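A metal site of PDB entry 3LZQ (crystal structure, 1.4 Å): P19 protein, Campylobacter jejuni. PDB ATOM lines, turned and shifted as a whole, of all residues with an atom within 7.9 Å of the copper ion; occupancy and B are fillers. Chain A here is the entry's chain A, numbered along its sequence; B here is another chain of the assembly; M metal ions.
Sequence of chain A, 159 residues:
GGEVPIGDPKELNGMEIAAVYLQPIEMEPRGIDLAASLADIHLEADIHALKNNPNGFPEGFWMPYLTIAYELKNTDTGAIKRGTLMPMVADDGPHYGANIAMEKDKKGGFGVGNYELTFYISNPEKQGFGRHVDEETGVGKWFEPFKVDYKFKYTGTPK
The copper ion is bound by a ring nitrogen (NE2) of His 42 (2.0 Å), a ring nitrogen (NE2) of His 132 of chain B (2.0 Å), a ring nitrogen (NE2) of His 95 (2.1 Å) and the side-chain sulfur (SD) of Met 88 (2.2 Å).
ND1 of His 42 sits at hydrogen-bond distance from OD1 of Asn 99 (2.9 Å). The backbone carbonyl oxygen (O) of Leu 22 lies within hydrogen-bond range of the backbone NH (N) of His 42 (2.8 Å). The backbone NH (N) of His 132 of chain B lies within hydrogen-bond range of the backbone carbonyl oxygen (O) of Val 89 (2.9 Å). A ring nitrogen (ND1) of His 132 of chain B lies within hydrogen-bond range of the side-chain hydroxyl (OG1) of Thr 137 of chain B, 2.9 Å away. NE2 of His 95 sits close to OE2 of Glu 44, at 3.3 Å.
Four residues have an atom within 4 Å of the copper ion: His 42, Met 88, His 95 and His 132 of chain B. The nearest printed residue that does not touch the copper ion is Glu 44 (4.02 Å).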
ATOM      1  N   LEU A  22      -5.027  20.866  23.768  1.00  0.00           N
ATOM      2  CA  LEU A  22      -4.053  21.890  23.566  1.00  0.00           C
ATOM      3  C   LEU A  22      -4.611  22.881  22.539  1.00  0.00           C
ATOM      4  O   LEU A  22      -5.746  22.837  22.160  1.00  0.00           O
ATOM      5  CB  LEU A  22      -2.695  21.300  23.212  1.00  0.00           C
ATOM      6  CG  LEU A  22      -2.606  20.376  22.043  1.00  0.00           C
ATOM      7  CD1 LEU A  22      -1.202  20.459  21.477  1.00  0.00           C
ATOM      8  CD2 LEU A  22      -2.934  18.952  22.416  1.00  0.00           C
ATOM      9  N   ILE A  25      -4.027  22.706  16.060  1.00  0.00           N
ATOM     10  CA  ILE A  25      -2.811  22.340  15.272  1.00  0.00           C
ATOM     11  C   ILE A  25      -3.139  22.281  13.784  1.00  0.00           C
ATOM     12  O   ILE A  25      -4.291  22.380  13.394  1.00  0.00           O
ATOM     13  CB  ILE A  25      -2.208  20.988  15.752  1.00  0.00           C
ATOM     14  CG1 ILE A  25      -3.193  19.826  15.607  1.00  0.00           C
ATOM     15  CG2 ILE A  25      -1.824  21.127  17.226  1.00  0.00           C
ATOM     16  CD1 ILE A  25      -3.371  19.239  14.121  1.00  0.00           C
ATOM     17  N   GLU A  26      -2.110  22.241  12.957  1.00  0.00           N
ATOM     18  CA  GLU A  26      -2.273  22.140  11.502  1.00  0.00           C
ATOM     19  C   GLU A  26      -1.905  20.747  11.073  1.00  0.00           C
ATOM     20  O   GLU A  26      -0.764  20.314  11.306  1.00  0.00           O
ATOM     21  CB  GLU A  26      -1.339  23.111  10.786  1.00  0.00           C
ATOM     22  CG  GLU A  26      -1.507  24.576  11.153  1.00  0.00           C
ATOM     23  CD  GLU A  26      -0.446  25.471  10.504  1.00  0.00           C
ATOM     24  OE1 GLU A  26      -0.024  25.249   9.330  1.00  0.00           O
ATOM     25  OE2 GLU A  26      -0.036  26.436  11.176  1.00  0.00           O
ATOM     26  N   MET A  27      -2.858  20.019  10.490  1.00  0.00           N
ATOM     27  CA  MET A  27      -2.632  18.620  10.118  1.00  0.00           C
ATOM     28  C   MET A  27      -2.614  18.427   8.595  1.00  0.00           C
ATOM     29  O   MET A  27      -3.434  19.015   7.869  1.00  0.00           O
ATOM     30  CB  MET A  27      -3.712  17.707  10.713  1.00  0.00           C
ATOM     31  CG  MET A  27      -3.396  16.192  10.593  1.00  0.00           C
ATOM     32  SD  MET A  27      -4.747  15.078  11.001  1.00  0.00           S
ATOM     33  CE  MET A  27      -5.607  15.033   9.412  1.00  0.00           C
ATOM     34  N   ASP A  33      -9.168  17.125   9.004  1.00  0.00           N
ATOM     35  CA  ASP A  33      -9.294  17.717  10.341  1.00  0.00           C
ATOM     36  C   ASP A  33      -9.761  19.166  10.182  1.00  0.00           C
ATOM     37  O   ASP A  33      -9.302  19.865   9.268  1.00  0.00           O
ATOM     38  CB  ASP A  33      -7.938  17.676  11.044  1.00  0.00           C
ATOM     39  CG  ASP A  33      -8.023  17.981  12.550  1.00  0.00           C
ATOM     40  OD1 ASP A  33      -8.899  17.447  13.239  1.00  0.00           O
ATOM     41  OD2 ASP A  33      -7.161  18.747  13.031  1.00  0.00           O
ATOM     42  N   HIS A  42      -7.187  21.486  20.180  1.00  0.00           N
ATOM     43  CA  HIS A  42      -6.888  20.125  19.633  1.00  0.00           C
ATOM     44  C   HIS A  42      -7.052  19.162  20.768  1.00  0.00           C
ATOM     45  O   HIS A  42      -6.349  19.264  21.765  1.00  0.00           O
ATOM     46  CB  HIS A  42      -5.454  20.018  19.109  1.00  0.00           C
ATOM     47  CG  HIS A  42      -5.223  18.797  18.259  1.00  0.00           C
ATOM     48  ND1 HIS A  42      -5.890  18.617  17.068  1.00  0.00           N
ATOM     49  CD2 HIS A  42      -4.359  17.733  18.380  1.00  0.00           C
ATOM     50  CE1 HIS A  42      -5.482  17.491  16.508  1.00  0.00           C
ATOM     51  NE2 HIS A  42      -4.572  16.917  17.283  1.00  0.00           N
ATOM     52  N   LEU A  43      -8.035  18.254  20.644  1.00  0.00           N
ATOM     53  CA  LEU A  43      -8.354  17.213  21.616  1.00  0.00           C
ATOM     54  C   LEU A  43      -7.522  16.007  21.239  1.00  0.00           C
ATOM     55  O   LEU A  43      -7.549  15.552  20.069  1.00  0.00           O
ATOM     56  CB  LEU A  43      -9.834  16.859  21.567  1.00  0.00           C
ATOM     57  CG  LEU A  43     -10.259  15.698  22.469  1.00  0.00           C
ATOM     58  CD1 LEU A  43      -9.979  15.944  23.953  1.00  0.00           C
ATOM     59  CD2 LEU A  43     -11.729  15.465  22.245  1.00  0.00           C
ATOM     60  N   GLU A  44      -6.785  15.421  22.194  1.00  0.00           N
ATOM     61  CA  GLU A  44      -6.061  14.164  21.965  1.00  0.00           C
ATOM     62  C   GLU A  44      -6.498  13.095  22.983  1.00  0.00           C
ATOM     63  O   GLU A  44      -6.664  13.375  24.190  1.00  0.00           O
ATOM     64  CB  GLU A  44      -4.533  14.389  22.093  1.00  0.00           C
ATOM     65  CG  GLU A  44      -3.994  15.418  21.168  1.00  0.00           C
ATOM     66  CD  GLU A  44      -2.535  15.616  21.242  1.00  0.00           C
ATOM     67  OE1 GLU A  44      -1.858  15.104  22.167  1.00  0.00           O
ATOM     68  OE2 GLU A  44      -1.993  16.286  20.335  1.00  0.00           O
ATOM     69  N   ALA A  45      -6.572  11.847  22.511  1.00  0.00           N
ATOM     70  CA  ALA A  45      -6.671  10.644  23.324  1.00  0.00           C
ATOM     71  C   ALA A  45      -5.250  10.011  23.269  1.00  0.00           C
ATOM     72  O   ALA A  45      -4.694   9.763  22.166  1.00  0.00           O
ATOM     73  CB  ALA A  45      -7.661   9.684  22.738  1.00  0.00           C
ATOM     74  N   MET A  86      -8.835  11.110  14.937  1.00  0.00           N
ATOM     75  CA  MET A  86      -8.093  10.448  13.856  1.00  0.00           C
ATOM     76  C   MET A  86      -6.651  10.178  14.235  1.00  0.00           C
ATOM     77  O   MET A  86      -6.043  10.969  14.990  1.00  0.00           O
ATOM     78  CB  MET A  86      -8.142  11.320  12.624  1.00  0.00           C
ATOM     79  CG  MET A  86      -9.569  11.387  12.043  1.00  0.00           C
ATOM     80  SD  MET A  86     -10.240   9.788  11.464  1.00  0.00           S
ATOM     81  CE  MET A  86      -9.257   9.491   9.976  1.00  0.00           C
ATOM     82  N   PRO A  87      -6.071   9.081  13.740  1.00  0.00           N
ATOM     83  CA  PRO A  87      -4.676   8.808  14.039  1.00  0.00           C
ATOM     84  C   PRO A  87      -3.699   9.739  13.322  1.00  0.00           C
ATOM     85  O   PRO A  87      -3.849  10.003  12.153  1.00  0.00           O
ATOM     86  CB  PRO A  87      -4.478   7.365  13.566  1.00  0.00           C
ATOM     87  CG  PRO A  87      -5.469   7.211  12.448  1.00  0.00           C
ATOM     88  CD  PRO A  87      -6.659   8.043  12.873  1.00  0.00           C
ATOM     89  N   MET A  88      -2.731  10.239  14.078  1.00  0.00           N
ATOM     90  CA  MET A  88      -1.738  11.152  13.524  1.00  0.00           C
ATOM     91  C   MET A  88      -0.522  11.202  14.426  1.00  0.00           C
ATOM     92  O   MET A  88      -0.525  10.634  15.539  1.00  0.00           O
ATOM     93  CB  MET A  88      -2.392  12.535  13.431  1.00  0.00           C
ATOM     94  CG  MET A  88      -2.758  13.145  14.763  1.00  0.00           C
ATOM     95  SD  MET A  88      -3.605  14.701  14.570  1.00  0.00           S
ATOM     96  CE  MET A  88      -5.214  14.049  14.219  1.00  0.00           C
ATOM     97  N   VAL A  89       0.518  11.855  13.900  1.00  0.00           N
ATOM     98  CA  VAL A  89       1.783  12.007  14.645  1.00  0.00           C
ATOM     99  C   VAL A  89       2.151  13.498  14.826  1.00  0.00           C
ATOM    100  O   VAL A  89       1.972  14.312  13.922  1.00  0.00           O
ATOM    101  CB  VAL A  89       2.942  11.167  14.001  1.00  0.00           C
ATOM    102  CG1 VAL A  89       3.423  11.732  12.639  1.00  0.00           C
ATOM    103  CG2 VAL A  89       4.125  11.050  14.985  1.00  0.00           C
ATOM    104  N   ALA A  90       2.673  13.810  16.012  1.00  0.00           N
ATOM    105  CA  ALA A  90       3.170  15.138  16.406  1.00  0.00           C
ATOM    106  C   ALA A  90       4.558  14.921  16.988  1.00  0.00           C
ATOM    107  O   ALA A  90       5.049  13.778  16.996  1.00  0.00           O
ATOM    108  CB  ALA A  90       2.201  15.837  17.413  1.00  0.00           C
ATOM    109  N   ASP A  92       5.602  14.797  19.803  1.00  0.00           N
ATOM    110  CA  ASP A  92       5.499  13.905  20.968  1.00  0.00           C
ATOM    111  C   ASP A  92       4.911  12.528  20.660  1.00  0.00           C
ATOM    112  O   ASP A  92       4.572  11.791  21.564  1.00  0.00           O
ATOM    113  CB  ASP A  92       4.824  14.572  22.165  1.00  0.00           C
ATOM    114  CG  ASP A  92       3.411  15.018  21.912  1.00  0.00           C
ATOM    115  OD1 ASP A  92       2.880  14.913  20.785  1.00  0.00           O
ATOM    116  OD2 ASP A  92       2.801  15.492  22.908  1.00  0.00           O
ATOM    117  N   GLY A  93       4.847  12.162  19.382  1.00  0.00           N
ATOM    118  CA  GLY A  93       4.556  10.824  18.969  1.00  0.00           C
ATOM    119  C   GLY A  93       3.157  10.665  18.451  1.00  0.00           C
ATOM    120  O   GLY A  93       2.412  11.654  18.340  1.00  0.00           O
ATOM    121  N   PRO A  94       2.755   9.401  18.175  1.00  0.00           N
ATOM    122  CA  PRO A  94       1.426   9.201  17.609  1.00  0.00           C
ATOM    123  C   PRO A  94       0.350   9.336  18.679  1.00  0.00           C
ATOM    124  O   PRO A  94       0.610   9.074  19.891  1.00  0.00           O
ATOM    125  CB  PRO A  94       1.480   7.780  17.109  1.00  0.00           C
ATOM    126  CG  PRO A  94       2.444   7.062  18.045  1.00  0.00           C
ATOM    127  CD  PRO A  94       3.515   8.130  18.259  1.00  0.00           C
ATOM    128  N   HIS A  95      -0.816   9.804  18.243  1.00  0.00           N
ATOM    129  CA  HIS A  95      -2.013   9.866  19.074  1.00  0.00           C
ATOM    130  C   HIS A  95      -3.255   9.831  18.193  1.00  0.00           C
ATOM    131  O   HIS A  95      -3.154   9.671  16.957  1.00  0.00           O
ATOM    132  CB  HIS A  95      -2.011  11.159  19.913  1.00  0.00           C
ATOM    133  CG  HIS A  95      -2.008  12.408  19.093  1.00  0.00           C
ATOM    134  ND1 HIS A  95      -0.853  13.054  18.746  1.00  0.00           N
ATOM    135  CD2 HIS A  95      -3.040  13.147  18.594  1.00  0.00           C
ATOM    136  CE1 HIS A  95      -1.171  14.125  18.022  1.00  0.00           C
ATOM    137  NE2 HIS A  95      -2.486  14.151  17.869  1.00  0.00           N
ATOM    138  N   TYR A  96      -4.422  10.001  18.819  1.00  0.00           N
ATOM    139  CA  TYR A  96      -5.678  10.154  18.099  1.00  0.00           C
ATOM    140  C   TYR A  96      -6.147  11.535  18.488  1.00  0.00           C
ATOM    141  O   TYR A  96      -6.185  11.869  19.697  1.00  0.00           O
ATOM    142  CB  TYR A  96      -6.716   9.112  18.537  1.00  0.00           C
ATOM    143  CG  TYR A  96      -6.314   7.683  18.254  1.00  0.00           C
ATOM    144  CD1 TYR A  96      -6.595   7.044  17.014  1.00  0.00           C
ATOM    145  CD2 TYR A  96      -5.655   6.957  19.204  1.00  0.00           C
ATOM    146  CE1 TYR A  96      -6.190   5.738  16.751  1.00  0.00           C
ATOM    147  CE2 TYR A  96      -5.270   5.656  18.983  1.00  0.00           C
ATOM    148  CZ  TYR A  96      -5.565   5.014  17.740  1.00  0.00           C
ATOM    149  OH  TYR A  96      -5.220   3.745  17.378  1.00  0.00           O
ATOM    150  N   GLY A  97      -6.521  12.348  17.516  1.00  0.00           N
ATOM    151  CA  GLY A  97      -6.855  13.716  17.812  1.00  0.00           C
ATOM    152  C   GLY A  97      -7.842  14.352  16.853  1.00  0.00           C
ATOM    153  O   GLY A  97      -8.190  13.784  15.817  1.00  0.00           O
ATOM    154  N   ALA A  98      -8.343  15.494  17.258  1.00  0.00           N
ATOM    155  CA  ALA A  98      -9.190  16.343  16.424  1.00  0.00           C
ATOM    156  C   ALA A  98      -9.174  17.789  16.863  1.00  0.00           C
ATOM    157  O   ALA A  98      -9.231  18.099  18.057  1.00  0.00           O
ATOM    158  CB  ALA A  98     -10.611  15.858  16.446  1.00  0.00           C
ATOM    159  N   ASN A  99      -9.114  18.686  15.884  1.00  0.00           N
ATOM    160  CA  ASN A  99      -9.387  20.118  16.107  1.00  0.00           C
ATOM    161  C   ASN A  99     -10.878  20.289  16.344  1.00  0.00           C
ATOM    162  O   ASN A  99     -11.707  19.666  15.662  1.00  0.00           O
ATOM    163  CB  ASN A  99      -8.903  21.006  14.944  1.00  0.00           C
ATOM    164  CG  ASN A  99      -7.452  21.381  15.018  1.00  0.00           C
ATOM    165  OD1 ASN A  99      -6.701  21.150  15.954  1.00  0.00           O
ATOM    166  ND2 ASN A  99      -7.050  22.028  13.947  1.00  0.00           N
ATOM    167  N   GLY B 130      -2.268  10.997   9.772  1.00  0.00           N
ATOM    168  CA  GLY B 130      -1.977  12.411   9.666  1.00  0.00           C
ATOM    169  C   GLY B 130      -0.709  12.810  10.379  1.00  0.00           C
ATOM    170  O   GLY B 130      -0.095  12.006  11.094  1.00  0.00           O
ATOM    171  N   ARG B 131      -0.255  14.034  10.101  1.00  0.00           N
ATOM    172  CA  ARG B 131       0.910  14.592  10.795  1.00  0.00           C
ATOM    173  C   ARG B 131       0.683  16.049  11.078  1.00  0.00           C
ATOM    174  O   ARG B 131       0.146  16.788  10.229  1.00  0.00           O
ATOM    175  CB  ARG B 131       2.251  14.376  10.055  1.00  0.00           C
ATOM    176  CG  ARG B 131       2.497  15.223   8.886  1.00  0.00           C
ATOM    177  CD  ARG B 131       3.838  14.935   8.285  1.00  0.00           C
ATOM    178  NE  ARG B 131       3.910  15.740   7.075  1.00  0.00           N
ATOM    179  CZ  ARG B 131       4.617  16.855   6.915  1.00  0.00           C
ATOM    180  NH1 ARG B 131       5.416  17.335   7.872  1.00  0.00           N
ATOM    181  NH2 ARG B 131       4.558  17.490   5.760  1.00  0.00           N
ATOM    182  N   HIS B 132       1.109  16.474  12.269  1.00  0.00           N
ATOM    183  CA  HIS B 132       1.073  17.874  12.613  1.00  0.00           C
ATOM    184  C   HIS B 132       2.184  18.536  11.806  1.00  0.00           C
ATOM    185  O   HIS B 132       3.274  17.996  11.689  1.00  0.00           O
ATOM    186  CB  HIS B 132       1.295  18.099  14.111  1.00  0.00           C
ATOM    187  CG  HIS B 132       0.204  17.593  15.008  1.00  0.00           C
ATOM    188  ND1 HIS B 132       0.005  18.079  16.278  1.00  0.00           N
ATOM    189  CD2 HIS B 132      -0.774  16.699  14.793  1.00  0.00           C
ATOM    190  CE1 HIS B 132      -0.993  17.415  16.859  1.00  0.00           C
ATOM    191  NE2 HIS B 132      -1.513  16.601  15.944  1.00  0.00           N
ATOM    192  N   ASP B 134       2.317  22.317  12.078  1.00  0.00           N
ATOM    193  CA  ASP B 134       2.494  23.606  12.745  1.00  0.00           C
ATOM    194  C   ASP B 134       3.897  23.707  13.401  1.00  0.00           C
ATOM    195  O   ASP B 134       4.573  22.694  13.687  1.00  0.00           O
ATOM    196  CB  ASP B 134       1.410  23.860  13.767  1.00  0.00           C
ATOM    197  CG  ASP B 134       1.228  22.709  14.691  1.00  0.00           C
ATOM    198  OD1 ASP B 134       0.635  21.720  14.192  1.00  0.00           O
ATOM    199  OD2 ASP B 134       1.729  22.764  15.844  1.00  0.00           O
ATOM    200  N   THR B 137       4.209  22.079  17.172  1.00  0.00           N
ATOM    201  CA  THR B 137       4.103  20.640  17.412  1.00  0.00           C
ATOM    202  C   THR B 137       4.369  19.735  16.214  1.00  0.00           C
ATOM    203  O   THR B 137       4.286  18.501  16.310  1.00  0.00           O
ATOM    204  CB  THR B 137       2.701  20.292  17.952  1.00  0.00           C
ATOM    205  OG1 THR B 137       1.747  20.364  16.875  1.00  0.00           O
ATOM    206  CG2 THR B 137       2.309  21.287  19.034  1.00  0.00           C
HETATM  207 CU    CU M   1      -3.189  15.602  16.556  1.00  0.00          CU
HETATM  208 MN    MN M   2       0.200  15.301  23.258  1.00  0.00          MN
